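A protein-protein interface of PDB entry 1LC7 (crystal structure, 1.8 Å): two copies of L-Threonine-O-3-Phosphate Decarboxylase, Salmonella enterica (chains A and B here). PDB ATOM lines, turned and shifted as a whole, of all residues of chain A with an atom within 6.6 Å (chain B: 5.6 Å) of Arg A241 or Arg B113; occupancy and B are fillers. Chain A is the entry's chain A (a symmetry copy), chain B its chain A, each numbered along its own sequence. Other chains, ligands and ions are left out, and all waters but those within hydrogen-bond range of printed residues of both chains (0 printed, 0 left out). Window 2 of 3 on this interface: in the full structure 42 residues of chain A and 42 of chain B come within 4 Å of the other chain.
The guanidinium group (NH2) of Arg B113 lies within hydrogen-bond range of the backbone carbonyl oxygen (O) of Arg A241, 2.7 Å away.
OE1 of Gln B117 sits close to O of Gln A242 (3.1 Å).
The guanidinium group (NH2) of Arg B113 lies within hydrogen-bond range of the backbone carbonyl oxygen (O) of Gln A243, at 2.9 Å.
The guanidinium group (NH1) of Arg B113 is in salt-bridge range of the side-chain carboxylate (OE1) of Glu B110, 2.9 Å away.
Among the printed residues, merely in contact across the chains: Gln A242 with Arg B113 (3.4 Å), Met A244 with Phe B90 (3.6 Å) and Pro A245 with Glu B110 (3.6 Å).
Arg A241 touches one residue of chain B.
Of chain A, only Arg A241 (2.7 Å), Gln A242 (3.4 Å) and Gln A243 (2.9 Å) come within 4 Å of Arg B113.
Printed residues of chain B within 4 Å of Gln A242: Arg B113 (3.4 Å) and Gln B117 (3.1 Å).
Of the printed residues of chain A, Glu B110 touches Pro A245 (3.6 Å).
Of the printed residues of chain A, Gln B117 touches Gln A242.
Printed residues of chain A within 4 Å of Phe B90: Met A244.
Printed residues of chain B within 4 Å of Gln A243: Arg B113.
Tyr B111 touches none of the printed residues of chain A.
The nearest residue of chain B that does not touch Arg A241 is Gln B117 (5.2 Å).
The nearest residue of chain A that does not touch Arg B113 is Pro A245 (4.1 Å).
Of the 11 printed residues of chain A, 5 touch a printed residue of chain B.
Of the 11 printed residues of chain B, 4 touch a printed residue of chain A.
Printed residues of chain B that touch a printed residue of chain A: Phe B90, Glu B110, Arg B113 and Gln B117.
Hydrophobic or aromatic side chains of chain B that line the printed part of chain A: Phe B90.
Among the printed residues, 6 pairs touch across the chains.
Among the printed residues, no Asp or Glu carboxylate lies within 4 Å of a Lys or Arg side-chain nitrogen of the other chain.
No position is printed for both chains.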
ATOM      1  N   ALA A 234      -5.356  10.792  -8.986  1.00  0.00           N
ATOM      2  CA  ALA A 234      -6.560  11.599  -8.743  1.00  0.00           C
ATOM      3  C   ALA A 234      -6.577  12.291  -7.375  1.00  0.00           C
ATOM      4  O   ALA A 234      -6.916  13.474  -7.275  1.00  0.00           O
ATOM      5  CB  ALA A 234      -7.818  10.722  -8.899  1.00  0.00           C
ATOM      6  N   MET A 236      -4.020  13.131  -5.368  1.00  0.00           N
ATOM      7  CA  MET A 236      -3.042  14.208  -5.273  1.00  0.00           C
ATOM      8  C   MET A 236      -3.484  15.410  -6.102  1.00  0.00           C
ATOM      9  O   MET A 236      -3.218  16.558  -5.728  1.00  0.00           O
ATOM     10  CB  MET A 236      -1.657  13.736  -5.727  1.00  0.00           C
ATOM     11  CG  MET A 236      -0.976  12.845  -4.679  1.00  0.00           C
ATOM     12  SD  MET A 236      -0.603  13.731  -3.113  1.00  0.00           S
ATOM     13  CE  MET A 236       0.153  15.152  -3.769  1.00  0.00           C
ATOM     14  N   ALA A 237      -4.169  15.153  -7.216  1.00  0.00           N
ATOM     15  CA  ALA A 237      -4.627  16.237  -8.072  1.00  0.00           C
ATOM     16  C   ALA A 237      -5.621  17.051  -7.269  1.00  0.00           C
ATOM     17  O   ALA A 237      -5.651  18.275  -7.370  1.00  0.00           O
ATOM     18  CB  ALA A 237      -5.288  15.696  -9.322  1.00  0.00           C
ATOM     19  N   ARG A 238      -6.410  16.363  -6.442  1.00  0.00           N
ATOM     20  CA  ARG A 238      -7.419  17.021  -5.610  1.00  0.00           C
ATOM     21  C   ARG A 238      -6.749  17.866  -4.533  1.00  0.00           C
ATOM     22  O   ARG A 238      -7.147  19.003  -4.285  1.00  0.00           O
ATOM     23  CB  ARG A 238      -8.338  15.988  -4.959  1.00  0.00           C
ATOM     24  CG  ARG A 238      -9.510  16.617  -4.233  1.00  0.00           C
ATOM     25  CD  ARG A 238     -10.559  15.598  -3.805  1.00  0.00           C
ATOM     26  NE  ARG A 238     -10.110  14.661  -2.770  1.00  0.00           N
ATOM     27  CZ  ARG A 238      -9.895  13.362  -2.984  1.00  0.00           C
ATOM     28  NH1 ARG A 238      -9.507  12.588  -1.990  1.00  0.00           N
ATOM     29  NH2 ARG A 238     -10.067  12.840  -4.197  1.00  0.00           N
ATOM     30  N   MET A 239      -5.710  17.312  -3.905  1.00  0.00           N
ATOM     31  CA  MET A 239      -4.957  18.042  -2.876  1.00  0.00           C
ATOM     32  C   MET A 239      -4.381  19.315  -3.528  1.00  0.00           C
ATOM     33  O   MET A 239      -4.363  20.371  -2.906  1.00  0.00           O
ATOM     34  CB  MET A 239      -3.779  17.195  -2.329  1.00  0.00           C
ATOM     35  CG  MET A 239      -4.129  15.869  -1.647  1.00  0.00           C
ATOM     36  SD  MET A 239      -4.949  16.137  -0.054  1.00  0.00           S
ATOM     37  CE  MET A 239      -5.512  14.444   0.367  1.00  0.00           C
ATOM     38  N   ARG A 240      -3.900  19.208  -4.767  1.00  0.00           N
ATOM     39  CA  ARG A 240      -3.329  20.373  -5.440  1.00  0.00           C
ATOM     40  C   ARG A 240      -4.361  21.410  -5.825  1.00  0.00           C
ATOM     41  O   ARG A 240      -4.122  22.617  -5.684  1.00  0.00           O
ATOM     42  CB  ARG A 240      -2.596  19.997  -6.714  1.00  0.00           C
ATOM     43  CG  ARG A 240      -1.270  19.339  -6.501  1.00  0.00           C
ATOM     44  CD  ARG A 240      -0.572  19.184  -7.823  1.00  0.00           C
ATOM     45  NE  ARG A 240       0.170  17.931  -7.750  1.00  0.00           N
ATOM     46  CZ  ARG A 240       1.334  17.814  -7.141  1.00  0.00           C
ATOM     47  NH1 ARG A 240       1.904  18.886  -6.575  1.00  0.00           N
ATOM     48  NH2 ARG A 240       1.893  16.616  -7.052  1.00  0.00           N
ATOM     49  N   ARG A 241      -5.507  20.988  -6.343  1.00  0.00           N
ATOM     50  CA  ARG A 241      -6.445  22.035  -6.724  1.00  0.00           C
ATOM     51  C   ARG A 241      -7.139  22.689  -5.549  1.00  0.00           C
ATOM     52  O   ARG A 241      -7.628  23.812  -5.676  1.00  0.00           O
ATOM     53  CB  ARG A 241      -7.478  21.548  -7.729  1.00  0.00           C
ATOM     54  CG  ARG A 241      -8.333  20.442  -7.282  1.00  0.00           C
ATOM     55  CD  ARG A 241      -9.467  20.275  -8.275  1.00  0.00           C
ATOM     56  NE  ARG A 241     -10.057  18.964  -8.100  1.00  0.00           N
ATOM     57  CZ  ARG A 241      -9.585  17.854  -8.656  1.00  0.00           C
ATOM     58  NH1 ARG A 241      -8.516  17.887  -9.445  1.00  0.00           N
ATOM     59  NH2 ARG A 241     -10.168  16.703  -8.394  1.00  0.00           N
ATOM     60  N   GLN A 242      -7.152  22.020  -4.400  1.00  0.00           N
ATOM     61  CA  GLN A 242      -7.805  22.575  -3.215  1.00  0.00           C
ATOM     62  C   GLN A 242      -6.853  23.332  -2.309  1.00  0.00           C
ATOM     63  O   GLN A 242      -7.269  23.910  -1.314  1.00  0.00           O
ATOM     64  CB  GLN A 242      -8.474  21.449  -2.408  1.00  0.00           C
ATOM     65  CG  GLN A 242      -9.432  20.630  -3.238  1.00  0.00           C
ATOM     66  CD  GLN A 242     -10.163  19.562  -2.451  1.00  0.00           C
ATOM     67  OE1 GLN A 242      -9.745  19.188  -1.359  1.00  0.00           O
ATOM     68  NE2 GLN A 242     -11.260  19.048  -3.023  1.00  0.00           N
ATOM     69  N   GLN A 243      -5.580  23.369  -2.670  1.00  0.00           N
ATOM     70  CA  GLN A 243      -4.602  24.004  -1.808  1.00  0.00           C
ATOM     71  C   GLN A 243      -4.631  25.538  -1.787  1.00  0.00           C
ATOM     72  O   GLN A 243      -5.274  26.177  -2.634  1.00  0.00           O
ATOM     73  CB  GLN A 243      -3.190  23.549  -2.187  1.00  0.00           C
ATOM     74  CG  GLN A 243      -2.585  24.243  -3.402  1.00  0.00           C
ATOM     75  CD  GLN A 243      -1.107  23.873  -3.601  1.00  0.00           C
ATOM     76  OE1 GLN A 243      -0.316  23.901  -2.655  1.00  0.00           O
ATOM     77  NE2 GLN A 243      -0.732  23.547  -4.834  1.00  0.00           N
ATOM     78  N   MET A 244      -3.921  26.102  -0.815  1.00  0.00           N
ATOM     79  CA  MET A 244      -3.812  27.550  -0.699  1.00  0.00           C
ATOM     80  C   MET A 244      -2.623  27.920  -1.573  1.00  0.00           C
ATOM     81  O   MET A 244      -1.574  27.292  -1.524  1.00  0.00           O
ATOM     82  CB  MET A 244      -3.535  27.971   0.733  1.00  0.00           C
ATOM     83  CG  MET A 244      -3.556  29.466   0.896  1.00  0.00           C
ATOM     84  SD  MET A 244      -3.416  29.976   2.641  1.00  0.00           S
ATOM     85  CE  MET A 244      -4.831  29.177   3.333  1.00  0.00           C
ATOM     86  N   PRO A 245      -2.759  28.978  -2.360  1.00  0.00           N
ATOM     87  CA  PRO A 245      -1.649  29.350  -3.222  1.00  0.00           C
ATOM     88  C   PRO A 245      -0.467  29.958  -2.492  1.00  0.00           C
ATOM     89  O   PRO A 245      -0.632  30.632  -1.465  1.00  0.00           O
ATOM     90  CB  PRO A 245      -2.293  30.325  -4.198  1.00  0.00           C
ATOM     91  CG  PRO A 245      -3.244  31.066  -3.303  1.00  0.00           C
ATOM     92  CD  PRO A 245      -3.873  29.939  -2.484  1.00  0.00           C
ATOM     93  N   PHE B  90      -8.615  33.028   3.941  1.00  0.00           N
ATOM     94  CA  PHE B  90      -9.104  31.706   4.348  1.00  0.00           C
ATOM     95  C   PHE B  90      -9.415  31.696   5.852  1.00  0.00           C
ATOM     96  O   PHE B  90     -10.379  31.045   6.302  1.00  0.00           O
ATOM     97  CB  PHE B  90      -8.083  30.606   3.989  1.00  0.00           C
ATOM     98  CG  PHE B  90      -8.177  30.155   2.545  1.00  0.00           C
ATOM     99  CD1 PHE B  90      -7.598  30.905   1.529  1.00  0.00           C
ATOM    100  CD2 PHE B  90      -8.903  29.011   2.200  1.00  0.00           C
ATOM    101  CE1 PHE B  90      -7.740  30.531   0.193  1.00  0.00           C
ATOM    102  CE2 PHE B  90      -9.055  28.627   0.863  1.00  0.00           C
ATOM    103  CZ  PHE B  90      -8.474  29.383  -0.139  1.00  0.00           C
ATOM    104  N   ALA B 109      -9.842  36.063  -6.963  1.00  0.00           N
ATOM    105  CA  ALA B 109     -10.471  34.733  -6.956  1.00  0.00           C
ATOM    106  C   ALA B 109     -10.524  33.976  -5.635  1.00  0.00           C
ATOM    107  O   ALA B 109     -11.403  33.132  -5.427  1.00  0.00           O
ATOM    108  CB  ALA B 109      -9.801  33.841  -8.007  1.00  0.00           C
ATOM    109  N   GLU B 110      -9.604  34.279  -4.730  1.00  0.00           N
ATOM    110  CA  GLU B 110      -9.568  33.523  -3.500  1.00  0.00           C
ATOM    111  C   GLU B 110     -10.776  33.663  -2.581  1.00  0.00           C
ATOM    112  O   GLU B 110     -11.006  32.753  -1.780  1.00  0.00           O
ATOM    113  CB  GLU B 110      -8.264  33.802  -2.736  1.00  0.00           C
ATOM    114  CG  GLU B 110      -6.991  33.369  -3.522  1.00  0.00           C
ATOM    115  CD  GLU B 110      -6.971  31.895  -3.900  1.00  0.00           C
ATOM    116  OE1 GLU B 110      -7.486  31.070  -3.098  1.00  0.00           O
ATOM    117  OE2 GLU B 110      -6.400  31.536  -4.986  1.00  0.00           O
ATOM    118  N   TYR B 111     -11.547  34.751  -2.661  1.00  0.00           N
ATOM    119  CA  TYR B 111     -12.713  34.872  -1.769  1.00  0.00           C
ATOM    120  C   TYR B 111     -13.666  33.709  -2.064  1.00  0.00           C
ATOM    121  O   TYR B 111     -14.143  33.033  -1.153  1.00  0.00           O
ATOM    122  CB  TYR B 111     -13.473  36.208  -1.984  1.00  0.00           C
ATOM    123  CG  TYR B 111     -12.622  37.469  -2.033  1.00  0.00           C
ATOM    124  CD1 TYR B 111     -11.696  37.763  -1.032  1.00  0.00           C
ATOM    125  CD2 TYR B 111     -12.771  38.392  -3.081  1.00  0.00           C
ATOM    126  CE1 TYR B 111     -10.926  38.959  -1.075  1.00  0.00           C
ATOM    127  CE2 TYR B 111     -12.017  39.582  -3.133  1.00  0.00           C
ATOM    128  CZ  TYR B 111     -11.101  39.853  -2.126  1.00  0.00           C
ATOM    129  OH  TYR B 111     -10.375  41.024  -2.179  1.00  0.00           O
ATOM    130  N   GLY B 112     -13.952  33.507  -3.345  1.00  0.00           N
ATOM    131  CA  GLY B 112     -14.840  32.434  -3.760  1.00  0.00           C
ATOM    132  C   GLY B 112     -14.272  31.071  -3.425  1.00  0.00           C
ATOM    133  O   GLY B 112     -15.015  30.151  -3.059  1.00  0.00           O
ATOM    134  N   ARG B 113     -12.954  30.916  -3.547  1.00  0.00           N
ATOM    135  CA  ARG B 113     -12.352  29.629  -3.220  1.00  0.00           C
ATOM    136  C   ARG B 113     -12.500  29.329  -1.755  1.00  0.00           C
ATOM    137  O   ARG B 113     -12.907  28.221  -1.383  1.00  0.00           O
ATOM    138  CB  ARG B 113     -10.849  29.567  -3.613  1.00  0.00           C
ATOM    139  CG  ARG B 113     -10.615  29.525  -5.097  1.00  0.00           C
ATOM    140  CD  ARG B 113      -9.157  29.219  -5.487  1.00  0.00           C
ATOM    141  NE  ARG B 113      -8.792  27.813  -5.266  1.00  0.00           N
ATOM    142  CZ  ARG B 113      -7.990  27.380  -4.292  1.00  0.00           C
ATOM    143  NH1 ARG B 113      -7.447  28.229  -3.427  1.00  0.00           N
ATOM    144  NH2 ARG B 113      -7.718  26.081  -4.187  1.00  0.00           N
ATOM    145  N   ALA B 114     -12.167  30.305  -0.908  1.00  0.00           N
ATOM    146  CA  ALA B 114     -12.264  30.120   0.538  1.00  0.00           C
ATOM    147  C   ALA B 114     -13.704  29.848   0.977  1.00  0.00           C
ATOM    148  O   ALA B 114     -13.938  28.985   1.834  1.00  0.00           O
ATOM    149  CB  ALA B 114     -11.724  31.362   1.276  1.00  0.00           C
ATOM    150  N   LEU B 115     -14.660  30.566   0.392  1.00  0.00           N
ATOM    151  CA  LEU B 115     -16.079  30.389   0.766  1.00  0.00           C
ATOM    152  C   LEU B 115     -16.653  29.051   0.315  1.00  0.00           C
ATOM    153  O   LEU B 115     -17.446  28.444   1.038  1.00  0.00           O
ATOM    154  CB  LEU B 115     -16.928  31.513   0.188  1.00  0.00           C
ATOM    155  CG  LEU B 115     -16.651  32.850   0.897  1.00  0.00           C
ATOM    156  CD1 LEU B 115     -17.295  33.976   0.111  1.00  0.00           C
ATOM    157  CD2 LEU B 115     -17.180  32.818   2.341  1.00  0.00           C
ATOM    158  N   ALA B 116     -16.264  28.609  -0.878  1.00  0.00           N
ATOM    159  CA  ALA B 116     -16.740  27.337  -1.397  1.00  0.00           C
ATOM    160  C   ALA B 116     -16.279  26.220  -0.470  1.00  0.00           C
ATOM    161  O   ALA B 116     -17.062  25.344  -0.081  1.00  0.00           O
ATOM    162  CB  ALA B 116     -16.204  27.103  -2.808  1.00  0.00           C
ATOM    163  N   GLN B 117     -15.007  26.249  -0.107  1.00  0.00           N
ATOM    164  CA  GLN B 117     -14.479  25.213   0.768  1.00  0.00           C
ATOM    165  C   GLN B 117     -15.103  25.253   2.152  1.00  0.00           C
ATOM    166  O   GLN B 117     -15.141  24.235   2.844  1.00  0.00           O
ATOM    167  CB  GLN B 117     -12.957  25.331   0.883  1.00  0.00           C
ATOM    168  CG  GLN B 117     -12.256  25.163  -0.440  1.00  0.00           C
ATOM    169  CD  GLN B 117     -10.738  25.293  -0.309  1.00  0.00           C
ATOM    170  OE1 GLN B 117     -10.014  25.275  -1.312  1.00  0.00           O
ATOM    171  NE2 GLN B 117     -10.257  25.440   0.922  1.00  0.00           N
ATOM    172  N   SER B 118     -15.584  26.419   2.572  1.00  0.00           N
ATOM    173  CA  SER B 118     -16.209  26.503   3.884  1.00  0.00           C
ATOM    174  C   SER B 118     -17.695  26.124   3.841  1.00  0.00           C
ATOM    175  O   SER B 118     -18.368  26.189   4.865  1.00  0.00           O
ATOM    176  CB  SER B 118     -16.026  27.902   4.502  1.00  0.00           C
ATOM    177  OG  SER B 118     -16.799  28.891   3.843  1.00  0.00           O
